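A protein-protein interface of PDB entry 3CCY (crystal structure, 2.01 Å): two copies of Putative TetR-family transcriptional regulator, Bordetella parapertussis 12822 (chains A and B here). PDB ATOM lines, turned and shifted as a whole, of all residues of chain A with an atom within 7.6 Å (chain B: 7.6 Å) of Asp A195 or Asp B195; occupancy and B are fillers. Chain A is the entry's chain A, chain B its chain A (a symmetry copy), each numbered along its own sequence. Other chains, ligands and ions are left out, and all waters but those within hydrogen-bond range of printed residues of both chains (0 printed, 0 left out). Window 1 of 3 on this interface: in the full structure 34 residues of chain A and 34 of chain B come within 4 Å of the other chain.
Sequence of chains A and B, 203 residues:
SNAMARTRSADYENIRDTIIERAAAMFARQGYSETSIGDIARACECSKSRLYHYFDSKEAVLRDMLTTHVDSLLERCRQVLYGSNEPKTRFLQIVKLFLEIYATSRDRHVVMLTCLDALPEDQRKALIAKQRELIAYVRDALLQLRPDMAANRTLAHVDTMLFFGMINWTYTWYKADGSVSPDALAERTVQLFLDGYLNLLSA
N of Tyr A197 is in hydrogen-bond range of O of Leu B194 (3.3 Å).
The backbone carbonyl oxygen (O) of Asp B195 sits close to the backbone carbonyl oxygen (O) of Asp A195.
O of Leu A194 sits at hydrogen-bond distance from N of Tyr B197 (3.3 Å).
The backbone NH (N) of Leu B198 lies within hydrogen-bond range of the backbone carbonyl oxygen (O) of Leu A194, at 2.9 Å.
The backbone NH (N) of Leu A198 sits at hydrogen-bond distance from the backbone carbonyl oxygen (O) of Leu B194, at 2.9 Å.
The backbone NH (N) of Tyr A197 sits at hydrogen-bond distance from the backbone carbonyl oxygen (O) of Phe B193 (2.8 Å).
N of Tyr B197 sits at hydrogen-bond distance from O of Phe A193 (2.8 Å).
O of Asp B195 lies close to OD1 of Asn B199 (2.7 Å).
N of Gly B196 is in hydrogen-bond range of O of Gln B191 (3.3 Å).
The side-chain amino group (NZ) of Lys A88 is in salt-bridge range of the side-chain carboxylate (OD2) of Asp A195 (2.9 Å).
The backbone carbonyl oxygen of Gln A191 sits at hydrogen-bond distance from the backbone NH of Gly A196 (3.3 Å).
OD1 of Asn A199 lies close to O of Asp A195 (2.7 Å).
The side-chain carboxylate (OD2) of Asp B195 is in salt-bridge range of the side-chain amino group (NZ) of Lys B88 (2.9 Å).
Among the printed residues, pairs that only touch across the chains: Gly A196 with Leu B194 (3.4 Å), Leu A194 with Gly B196 (3.4 Å), Gly A196 with Phe B193 (3.5 Å), Phe A193 with Gly B196 (3.5 Å), Gly A196 with Gly B196 (3.5 Å), Lys A88 with Leu B198 (3.6 Å), Leu A198 with Lys B88 (3.6 Å), Asp A195 with Gly B196 (3.7 Å), Gly A196 with Asp B195 (3.7 Å), Asp A195 with Leu B198 (3.7 Å), Leu A198 with Asp B195 (3.7 Å), Leu A192 with Phe B193 (3.9 Å), Phe A193 with Leu B192 (3.9 Å), Asp A195 with Asn B199 (3.9 Å) and Asn A199 with Asp B195 (3.9 Å).
Of the printed residues of chain B, Asp A195 touches Asp B195 (3.3 Å), Gly B196 (3.7 Å), Leu B198 (3.7 Å) and Asn B199 (3.9 Å).
Asp B195 touches just these residues of chain A: Asp A195, Gly A196, Leu A198 and Asn A199.
Gly A196 touches four residues of chain B.
Of chain A, only Phe A193, Leu A194, Asp A195 and Gly A196 come within 4 Å of Gly B196.
Of the printed residues of chain A, Asn B199 touches Asp A195 (3.9 Å).
Of the printed residues of chain B, Tyr A197 touches Phe B193 and Leu B194.
Printed residues of chain B within 4 Å of Leu A198: Lys B88 (3.6 Å), Leu B194 (2.9 Å) and Asp B195 (3.7 Å).
Of the printed residues of chain B, Leu A194 touches Gly B196 (3.4 Å), Tyr B197 (3.3 Å) and Leu B198 (2.9 Å).
The nearest residue of chain A that does not touch Asp B195 is Leu A194 (4.6 Å).
Among the printed residues, no Asp or Glu carboxylate lies within 4 Å of a Lys or Arg side-chain nitrogen of the other chain.
Leu A194 touches Leu B198, and with the chains exchanged Leu A198 touches Leu B194.
Asp A195 touches its own counterpart, Asp B195.
Asp A195 touches Gly B196, and with the chains exchanged Gly A196 touches Asp B195.
Gly B196 touches its own counterpart, Gly A196.
13 positions are printed for both chains.
Of the 22 pairs that touch across the chains among the printed residues, 22 have their exchanged pair printed and touching as well.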
ATOM      1  N   LYS A  88       2.472 -15.852  20.066  1.00  0.00           N
ATOM      2  CA  LYS A  88       2.367 -17.319  19.951  1.00  0.00           C
ATOM      3  C   LYS A  88       3.751 -17.958  19.951  1.00  0.00           C
ATOM      4  O   LYS A  88       3.953 -19.016  20.572  1.00  0.00           O
ATOM      5  CB  LYS A  88       1.512 -17.807  18.764  1.00  0.00           C
ATOM      6  CG  LYS A  88       1.002 -19.281  18.962  1.00  0.00           C
ATOM      7  CD  LYS A  88      -0.211 -19.696  18.075  1.00  0.00           C
ATOM      8  CE  LYS A  88      -0.354 -21.240  18.026  1.00  0.00           C
ATOM      9  NZ  LYS A  88      -1.755 -21.784  17.697  1.00  0.00           N
ATOM     10  N   THR A 189       2.748 -30.392  23.360  1.00  0.00           N
ATOM     11  CA  THR A 189       2.136 -29.737  24.541  1.00  0.00           C
ATOM     12  C   THR A 189       1.408 -28.415  24.179  1.00  0.00           C
ATOM     13  O   THR A 189       0.250 -28.182  24.548  1.00  0.00           O
ATOM     14  CB  THR A 189       3.209 -29.470  25.600  1.00  0.00           C
ATOM     15  OG1 THR A 189       3.794 -30.730  25.965  1.00  0.00           O
ATOM     16  CG2 THR A 189       2.621 -28.772  26.846  1.00  0.00           C
ATOM     17  N   VAL A 190       2.079 -27.577  23.426  1.00  0.00           N
ATOM     18  CA  VAL A 190       1.469 -26.335  22.958  1.00  0.00           C
ATOM     19  C   VAL A 190       0.316 -26.517  21.973  1.00  0.00           C
ATOM     20  O   VAL A 190      -0.721 -25.854  22.120  1.00  0.00           O
ATOM     21  CB  VAL A 190       2.549 -25.406  22.356  1.00  0.00           C
ATOM     22  CG1 VAL A 190       1.926 -24.155  21.721  1.00  0.00           C
ATOM     23  CG2 VAL A 190       3.527 -24.992  23.452  1.00  0.00           C
ATOM     24  N   GLN A 191       0.489 -27.376  20.958  1.00  0.00           N
ATOM     25  CA  GLN A 191      -0.619 -27.660  20.020  1.00  0.00           C
ATOM     26  C   GLN A 191      -1.872 -28.150  20.815  1.00  0.00           C
ATOM     27  O   GLN A 191      -2.992 -27.700  20.574  1.00  0.00           O
ATOM     28  CB  GLN A 191      -0.194 -28.735  18.950  1.00  0.00           C
ATOM     29  CG  GLN A 191       0.906 -28.235  17.936  1.00  0.00           C
ATOM     30  CD  GLN A 191       1.703 -29.403  17.238  1.00  0.00           C
ATOM     31  OE1 GLN A 191       1.341 -30.610  17.350  1.00  0.00           O
ATOM     32  NE2 GLN A 191       2.812 -29.035  16.541  1.00  0.00           N
ATOM     33  N   LEU A 192      -1.668 -29.105  21.726  1.00  0.00           N
ATOM     34  CA  LEU A 192      -2.764 -29.664  22.517  1.00  0.00           C
ATOM     35  C   LEU A 192      -3.421 -28.578  23.377  1.00  0.00           C
ATOM     36  O   LEU A 192      -4.667 -28.409  23.341  1.00  0.00           O
ATOM     37  CB  LEU A 192      -2.256 -30.803  23.419  1.00  0.00           C
ATOM     38  CG  LEU A 192      -1.859 -32.153  22.797  1.00  0.00           C
ATOM     39  CD1 LEU A 192      -0.935 -32.922  23.771  1.00  0.00           C
ATOM     40  CD2 LEU A 192      -3.101 -33.000  22.507  1.00  0.00           C
ATOM     41  N   PHE A 193      -2.603 -27.874  24.161  1.00  0.00           N
ATOM     42  CA  PHE A 193      -3.115 -26.856  25.110  1.00  0.00           C
ATOM     43  C   PHE A 193      -3.833 -25.711  24.374  1.00  0.00           C
ATOM     44  O   PHE A 193      -4.920 -25.346  24.754  1.00  0.00           O
ATOM     45  CB  PHE A 193      -2.017 -26.271  26.030  1.00  0.00           C
ATOM     46  CG  PHE A 193      -2.587 -25.354  27.113  1.00  0.00           C
ATOM     47  CD1 PHE A 193      -3.272 -25.889  28.195  1.00  0.00           C
ATOM     48  CD2 PHE A 193      -2.492 -23.976  27.002  1.00  0.00           C
ATOM     49  CE1 PHE A 193      -3.843 -25.059  29.182  1.00  0.00           C
ATOM     50  CE2 PHE A 193      -3.059 -23.151  27.983  1.00  0.00           C
ATOM     51  CZ  PHE A 193      -3.731 -23.708  29.059  1.00  0.00           C
ATOM     52  N   LEU A 194      -3.222 -25.167  23.316  1.00  0.00           N
ATOM     53  CA  LEU A 194      -3.805 -24.032  22.586  1.00  0.00           C
ATOM     54  C   LEU A 194      -4.959 -24.395  21.650  1.00  0.00           C
ATOM     55  O   LEU A 194      -5.954 -23.680  21.572  1.00  0.00           O
ATOM     56  CB  LEU A 194      -2.722 -23.281  21.776  1.00  0.00           C
ATOM     57  CG  LEU A 194      -1.645 -22.584  22.625  1.00  0.00           C
ATOM     58  CD1 LEU A 194      -0.819 -21.688  21.718  1.00  0.00           C
ATOM     59  CD2 LEU A 194      -2.203 -21.770  23.813  1.00  0.00           C
ATOM     60  N   ASP A 195      -4.812 -25.492  20.923  1.00  0.00           N
ATOM     61  CA  ASP A 195      -5.770 -25.810  19.861  1.00  0.00           C
ATOM     62  C   ASP A 195      -6.624 -27.054  20.121  1.00  0.00           C
ATOM     63  O   ASP A 195      -7.660 -27.269  19.451  1.00  0.00           O
ATOM     64  CB  ASP A 195      -5.041 -25.857  18.505  1.00  0.00           C
ATOM     65  CG  ASP A 195      -4.541 -24.459  18.078  1.00  0.00           C
ATOM     66  OD1 ASP A 195      -5.393 -23.576  17.810  1.00  0.00           O
ATOM     67  OD2 ASP A 195      -3.321 -24.219  18.044  1.00  0.00           O
ATOM     68  N   GLY A 196      -6.234 -27.856  21.117  1.00  0.00           N
ATOM     69  CA  GLY A 196      -7.118 -28.942  21.549  1.00  0.00           C
ATOM     70  C   GLY A 196      -6.841 -30.284  20.925  1.00  0.00           C
ATOM     71  O   GLY A 196      -6.536 -30.384  19.747  1.00  0.00           O
ATOM     72  N   TYR A 197      -6.964 -31.334  21.745  1.00  0.00           N
ATOM     73  CA  TYR A 197      -6.856 -32.723  21.306  1.00  0.00           C
ATOM     74  C   TYR A 197      -7.719 -33.047  20.075  1.00  0.00           C
ATOM     75  O   TYR A 197      -7.286 -33.789  19.161  1.00  0.00           O
ATOM     76  CB  TYR A 197      -7.275 -33.639  22.453  1.00  0.00           C
ATOM     77  CG  TYR A 197      -7.044 -35.078  22.165  1.00  0.00           C
ATOM     78  CD1 TYR A 197      -8.112 -35.954  21.962  1.00  0.00           C
ATOM     79  CD2 TYR A 197      -5.760 -35.573  22.090  1.00  0.00           C
ATOM     80  CE1 TYR A 197      -7.871 -37.302  21.676  1.00  0.00           C
ATOM     81  CE2 TYR A 197      -5.519 -36.911  21.796  1.00  0.00           C
ATOM     82  CZ  TYR A 197      -6.570 -37.767  21.620  1.00  0.00           C
ATOM     83  OH  TYR A 197      -6.294 -39.113  21.300  1.00  0.00           O
ATOM     84  N   LEU A 198      -8.943 -32.523  20.076  1.00  0.00           N
ATOM     85  CA  LEU A 198      -9.895 -32.779  18.988  1.00  0.00           C
ATOM     86  C   LEU A 198      -9.545 -32.164  17.606  1.00  0.00           C
ATOM     87  O   LEU A 198     -10.099 -32.590  16.581  1.00  0.00           O
ATOM     88  CB  LEU A 198     -11.308 -32.411  19.426  1.00  0.00           C
ATOM     89  CG  LEU A 198     -11.912 -33.157  20.634  1.00  0.00           C
ATOM     90  CD1 LEU A 198     -13.349 -32.638  20.919  1.00  0.00           C
ATOM     91  CD2 LEU A 198     -11.960 -34.713  20.456  1.00  0.00           C
ATOM     92  N   ASN A 199      -8.613 -31.212  17.564  1.00  0.00           N
ATOM     93  CA  ASN A 199      -8.242 -30.573  16.288  1.00  0.00           C
ATOM     94  C   ASN A 199      -6.805 -30.894  15.854  1.00  0.00           C
ATOM     95  O   ASN A 199      -6.312 -30.389  14.836  1.00  0.00           O
ATOM     96  CB  ASN A 199      -8.414 -29.050  16.386  1.00  0.00           C
ATOM     97  CG  ASN A 199      -9.732 -28.662  16.985  1.00  0.00           C
ATOM     98  OD1 ASN A 199      -9.802 -28.167  18.120  1.00  0.00           O
ATOM     99  ND2 ASN A 199     -10.792 -28.915  16.262  1.00  0.00           N
ATOM    100  N   LEU A 200      -6.135 -31.716  16.639  1.00  0.00           N
ATOM    101  CA  LEU A 200      -4.758 -32.057  16.386  1.00  0.00           C
ATOM    102  C   LEU A 200      -4.747 -32.879  15.101  1.00  0.00           C
ATOM    103  O   LEU A 200      -5.595 -33.766  14.914  1.00  0.00           O
ATOM    104  CB  LEU A 200      -4.289 -32.912  17.554  1.00  0.00           C
ATOM    105  CG  LEU A 200      -2.936 -32.919  18.257  1.00  0.00           C
ATOM    106  CD1 LEU A 200      -2.315 -31.556  18.487  1.00  0.00           C
ATOM    107  CD2 LEU A 200      -3.170 -33.602  19.576  1.00  0.00           C
ATOM    108  N   LYS B  88     -17.761 -38.707  24.508  1.00  0.00           N
ATOM    109  CA  LYS B  88     -17.372 -37.402  25.077  1.00  0.00           C
ATOM    110  C   LYS B  88     -17.858 -37.279  26.517  1.00  0.00           C
ATOM    111  O   LYS B  88     -17.135 -36.751  27.379  1.00  0.00           O
ATOM    112  CB  LYS B  88     -17.788 -36.185  24.227  1.00  0.00           C
ATOM    113  CG  LYS B  88     -16.943 -34.903  24.566  1.00  0.00           C
ATOM    114  CD  LYS B  88     -16.960 -33.784  23.482  1.00  0.00           C
ATOM    115  CE  LYS B  88     -16.476 -32.435  24.076  1.00  0.00           C
ATOM    116  NZ  LYS B  88     -15.904 -31.415  23.077  1.00  0.00           N
ATOM    117  N   THR B 189     -10.907 -28.257  32.643  1.00  0.00           N
ATOM    118  CA  THR B 189      -9.831 -29.178  32.206  1.00  0.00           C
ATOM    119  C   THR B 189     -10.163 -29.892  30.869  1.00  0.00           C
ATOM    120  O   THR B 189      -9.364 -29.919  29.924  1.00  0.00           O
ATOM    121  CB  THR B 189      -9.562 -30.215  33.300  1.00  0.00           C
ATOM    122  OG1 THR B 189      -9.175 -29.513  34.490  1.00  0.00           O
ATOM    123  CG2 THR B 189      -8.456 -31.211  32.883  1.00  0.00           C
ATOM    124  N   VAL B 190     -11.356 -30.431  30.786  1.00  0.00           N
ATOM    125  CA  VAL B 190     -11.808 -31.063  29.549  1.00  0.00           C
ATOM    126  C   VAL B 190     -12.004 -30.108  28.373  1.00  0.00           C
ATOM    127  O   VAL B 190     -11.573 -30.423  27.254  1.00  0.00           O
ATOM    128  CB  VAL B 190     -13.103 -31.869  29.807  1.00  0.00           C
ATOM    129  CG1 VAL B 190     -13.690 -32.425  28.502  1.00  0.00           C
ATOM    130  CG2 VAL B 190     -12.800 -33.018  30.765  1.00  0.00           C
ATOM    131  N   GLN B 191     -12.670 -28.965  28.598  1.00  0.00           N
ATOM    132  CA  GLN B 191     -12.818 -27.961  27.522  1.00  0.00           C
ATOM    133  C   GLN B 191     -11.410 -27.560  26.976  1.00  0.00           C
ATOM    134  O   GLN B 191     -11.195 -27.491  25.766  1.00  0.00           O
ATOM    135  CB  GLN B 191     -13.589 -26.688  28.038  1.00  0.00           C
ATOM    136  CG  GLN B 191     -15.105 -26.949  28.384  1.00  0.00           C
ATOM    137  CD  GLN B 191     -15.724 -25.883  29.369  1.00  0.00           C
ATOM    138  OE1 GLN B 191     -15.100 -24.826  29.675  1.00  0.00           O
ATOM    139  NE2 GLN B 191     -16.945 -26.187  29.885  1.00  0.00           N
ATOM    140  N   LEU B 192     -10.478 -27.256  27.884  1.00  0.00           N
ATOM    141  CA  LEU B 192      -9.130 -26.842  27.498  1.00  0.00           C
ATOM    142  C   LEU B 192      -8.423 -27.957  26.719  1.00  0.00           C
ATOM    143  O   LEU B 192      -7.896 -27.715  25.604  1.00  0.00           O
ATOM    144  CB  LEU B 192      -8.301 -26.471  28.741  1.00  0.00           C
ATOM    145  CG  LEU B 192      -8.609 -25.172  29.506  1.00  0.00           C
ATOM    146  CD1 LEU B 192      -8.031 -25.264  30.938  1.00  0.00           C
ATOM    147  CD2 LEU B 192      -7.992 -23.965  28.792  1.00  0.00           C
ATOM    148  N   PHE B 193      -8.384 -29.153  27.309  1.00  0.00           N
ATOM    149  CA  PHE B 193      -7.653 -30.296  26.710  1.00  0.00           C
ATOM    150  C   PHE B 193      -8.246 -30.689  25.345  1.00  0.00           C
ATOM    151  O   PHE B 193      -7.512 -30.852  24.400  1.00  0.00           O
ATOM    152  CB  PHE B 193      -7.604 -31.540  27.630  1.00  0.00           C
ATOM    153  CG  PHE B 193      -6.706 -32.645  27.073  1.00  0.00           C
ATOM    154  CD1 PHE B 193      -5.325 -32.509  27.107  1.00  0.00           C
ATOM    155  CD2 PHE B 193      -7.249 -33.766  26.466  1.00  0.00           C
ATOM    156  CE1 PHE B 193      -4.479 -33.496  26.560  1.00  0.00           C
ATOM    157  CE2 PHE B 193      -6.408 -34.747  25.922  1.00  0.00           C
ATOM    158  CZ  PHE B 193      -5.033 -34.594  25.975  1.00  0.00           C
ATOM    159  N   LEU B 194      -9.574 -30.821  25.254  1.00  0.00           N
ATOM    160  CA  LEU B 194     -10.224 -31.250  24.007  1.00  0.00           C
ATOM    161  C   LEU B 194     -10.325 -30.167  22.932  1.00  0.00           C
ATOM    162  O   LEU B 194     -10.115 -30.431  21.752  1.00  0.00           O
ATOM    163  CB  LEU B 194     -11.638 -31.810  24.286  1.00  0.00           C
ATOM    164  CG  LEU B 194     -11.670 -33.108  25.113  1.00  0.00           C
ATOM    165  CD1 LEU B 194     -13.082 -33.667  25.081  1.00  0.00           C
ATOM    166  CD2 LEU B 194     -10.661 -34.180  24.648  1.00  0.00           C
ATOM    167  N   ASP B 195     -10.671 -28.955  23.339  1.00  0.00           N
ATOM    168  CA  ASP B 195     -10.984 -27.908  22.363  1.00  0.00           C
ATOM    169  C   ASP B 195      -9.989 -26.745  22.331  1.00  0.00           C
ATOM    170  O   ASP B 195      -9.972 -25.945  21.367  1.00  0.00           O
ATOM    171  CB  ASP B 195     -12.441 -27.444  22.553  1.00  0.00           C
ATOM    172  CG  ASP B 195     -13.447 -28.552  22.169  1.00  0.00           C
ATOM    173  OD1 ASP B 195     -13.512 -28.908  20.967  1.00  0.00           O
ATOM    174  OD2 ASP B 195     -14.140 -29.094  23.047  1.00  0.00           O
ATOM    175  N   GLY B 196      -9.123 -26.663  23.346  1.00  0.00           N
ATOM    176  CA  GLY B 196      -8.019 -25.704  23.269  1.00  0.00           C
ATOM    177  C   GLY B 196      -8.271 -24.376  23.931  1.00  0.00           C
ATOM    178  O   GLY B 196      -9.359 -23.827  23.854  1.00  0.00           O
ATOM    179  N   TYR B 197      -7.228 -23.854  24.587  1.00  0.00           N
ATOM    180  CA  TYR B 197      -7.233 -22.525  25.191  1.00  0.00           C
ATOM    181  C   TYR B 197      -7.730 -21.421  24.242  1.00  0.00           C
ATOM    182  O   TYR B 197      -8.474 -20.500  24.658  1.00  0.00           O
ATOM    183  CB  TYR B 197      -5.816 -22.181  25.644  1.00  0.00           C
ATOM    184  CG  TYR B 197      -5.742 -20.916  26.421  1.00  0.00           C
ATOM    185  CD1 TYR B 197      -5.131 -19.778  25.892  1.00  0.00           C
ATOM    186  CD2 TYR B 197      -6.284 -20.848  27.686  1.00  0.00           C
ATOM    187  CE1 TYR B 197      -5.087 -18.594  26.634  1.00  0.00           C
ATOM    188  CE2 TYR B 197      -6.249 -19.668  28.422  1.00  0.00           C
ATOM    189  CZ  TYR B 197      -5.629 -18.564  27.906  1.00  0.00           C
ATOM    190  OH  TYR B 197      -5.631 -17.376  28.666  1.00  0.00           O
ATOM    191  N   LEU B 198      -7.286 -21.497  22.989  1.00  0.00           N
ATOM    192  CA  LEU B 198      -7.643 -20.490  21.981  1.00  0.00           C
ATOM    193  C   LEU B 198      -9.131 -20.452  21.538  1.00  0.00           C
ATOM    194  O   LEU B 198      -9.578 -19.451  20.958  1.00  0.00           O
ATOM    195  CB  LEU B 198      -6.702 -20.587  20.784  1.00  0.00           C
ATOM    196  CG  LEU B 198      -5.196 -20.358  21.024  1.00  0.00           C
ATOM    197  CD1 LEU B 198      -4.414 -20.502  19.688  1.00  0.00           C
ATOM    198  CD2 LEU B 198      -4.860 -18.968  21.662  1.00  0.00           C
ATOM    199  N   ASN B 199      -9.899 -21.498  21.843  1.00  0.00           N
ATOM    200  CA  ASN B 199     -11.317 -21.536  21.440  1.00  0.00           C
ATOM    201  C   ASN B 199     -12.279 -21.487  22.634  1.00  0.00           C
ATOM    202  O   ASN B 199     -13.505 -21.572  22.478  1.00  0.00           O
ATOM    203  CB  ASN B 199     -11.600 -22.797  20.611  1.00  0.00           C
ATOM    204  CG  ASN B 199     -10.580 -23.015  19.535  1.00  0.00           C
ATOM    205  OD1 ASN B 199      -9.759 -23.941  19.605  1.00  0.00           O
ATOM    206  ND2 ASN B 199     -10.584 -22.151  18.553  1.00  0.00           N
ATOM    207  N   LEU B 200     -11.718 -21.372  23.823  1.00  0.00           N
ATOM    208  CA  LEU B 200     -12.496 -21.374  25.036  1.00  0.00           C
ATOM    209  C   LEU B 200     -13.317 -20.088  25.024  1.00  0.00           C
ATOM    210  O   LEU B 200     -12.796 -19.013  24.686  1.00  0.00           O
ATOM    211  CB  LEU B 200     -11.513 -21.353  26.197  1.00  0.00           C
ATOM    212  CG  LEU B 200     -11.592 -22.077  27.536  1.00  0.00           C
ATOM    213  CD1 LEU B 200     -12.106 -23.501  27.478  1.00  0.00           C
ATOM    214  CD2 LEU B 200     -10.192 -22.062  28.086  1.00  0.00           C
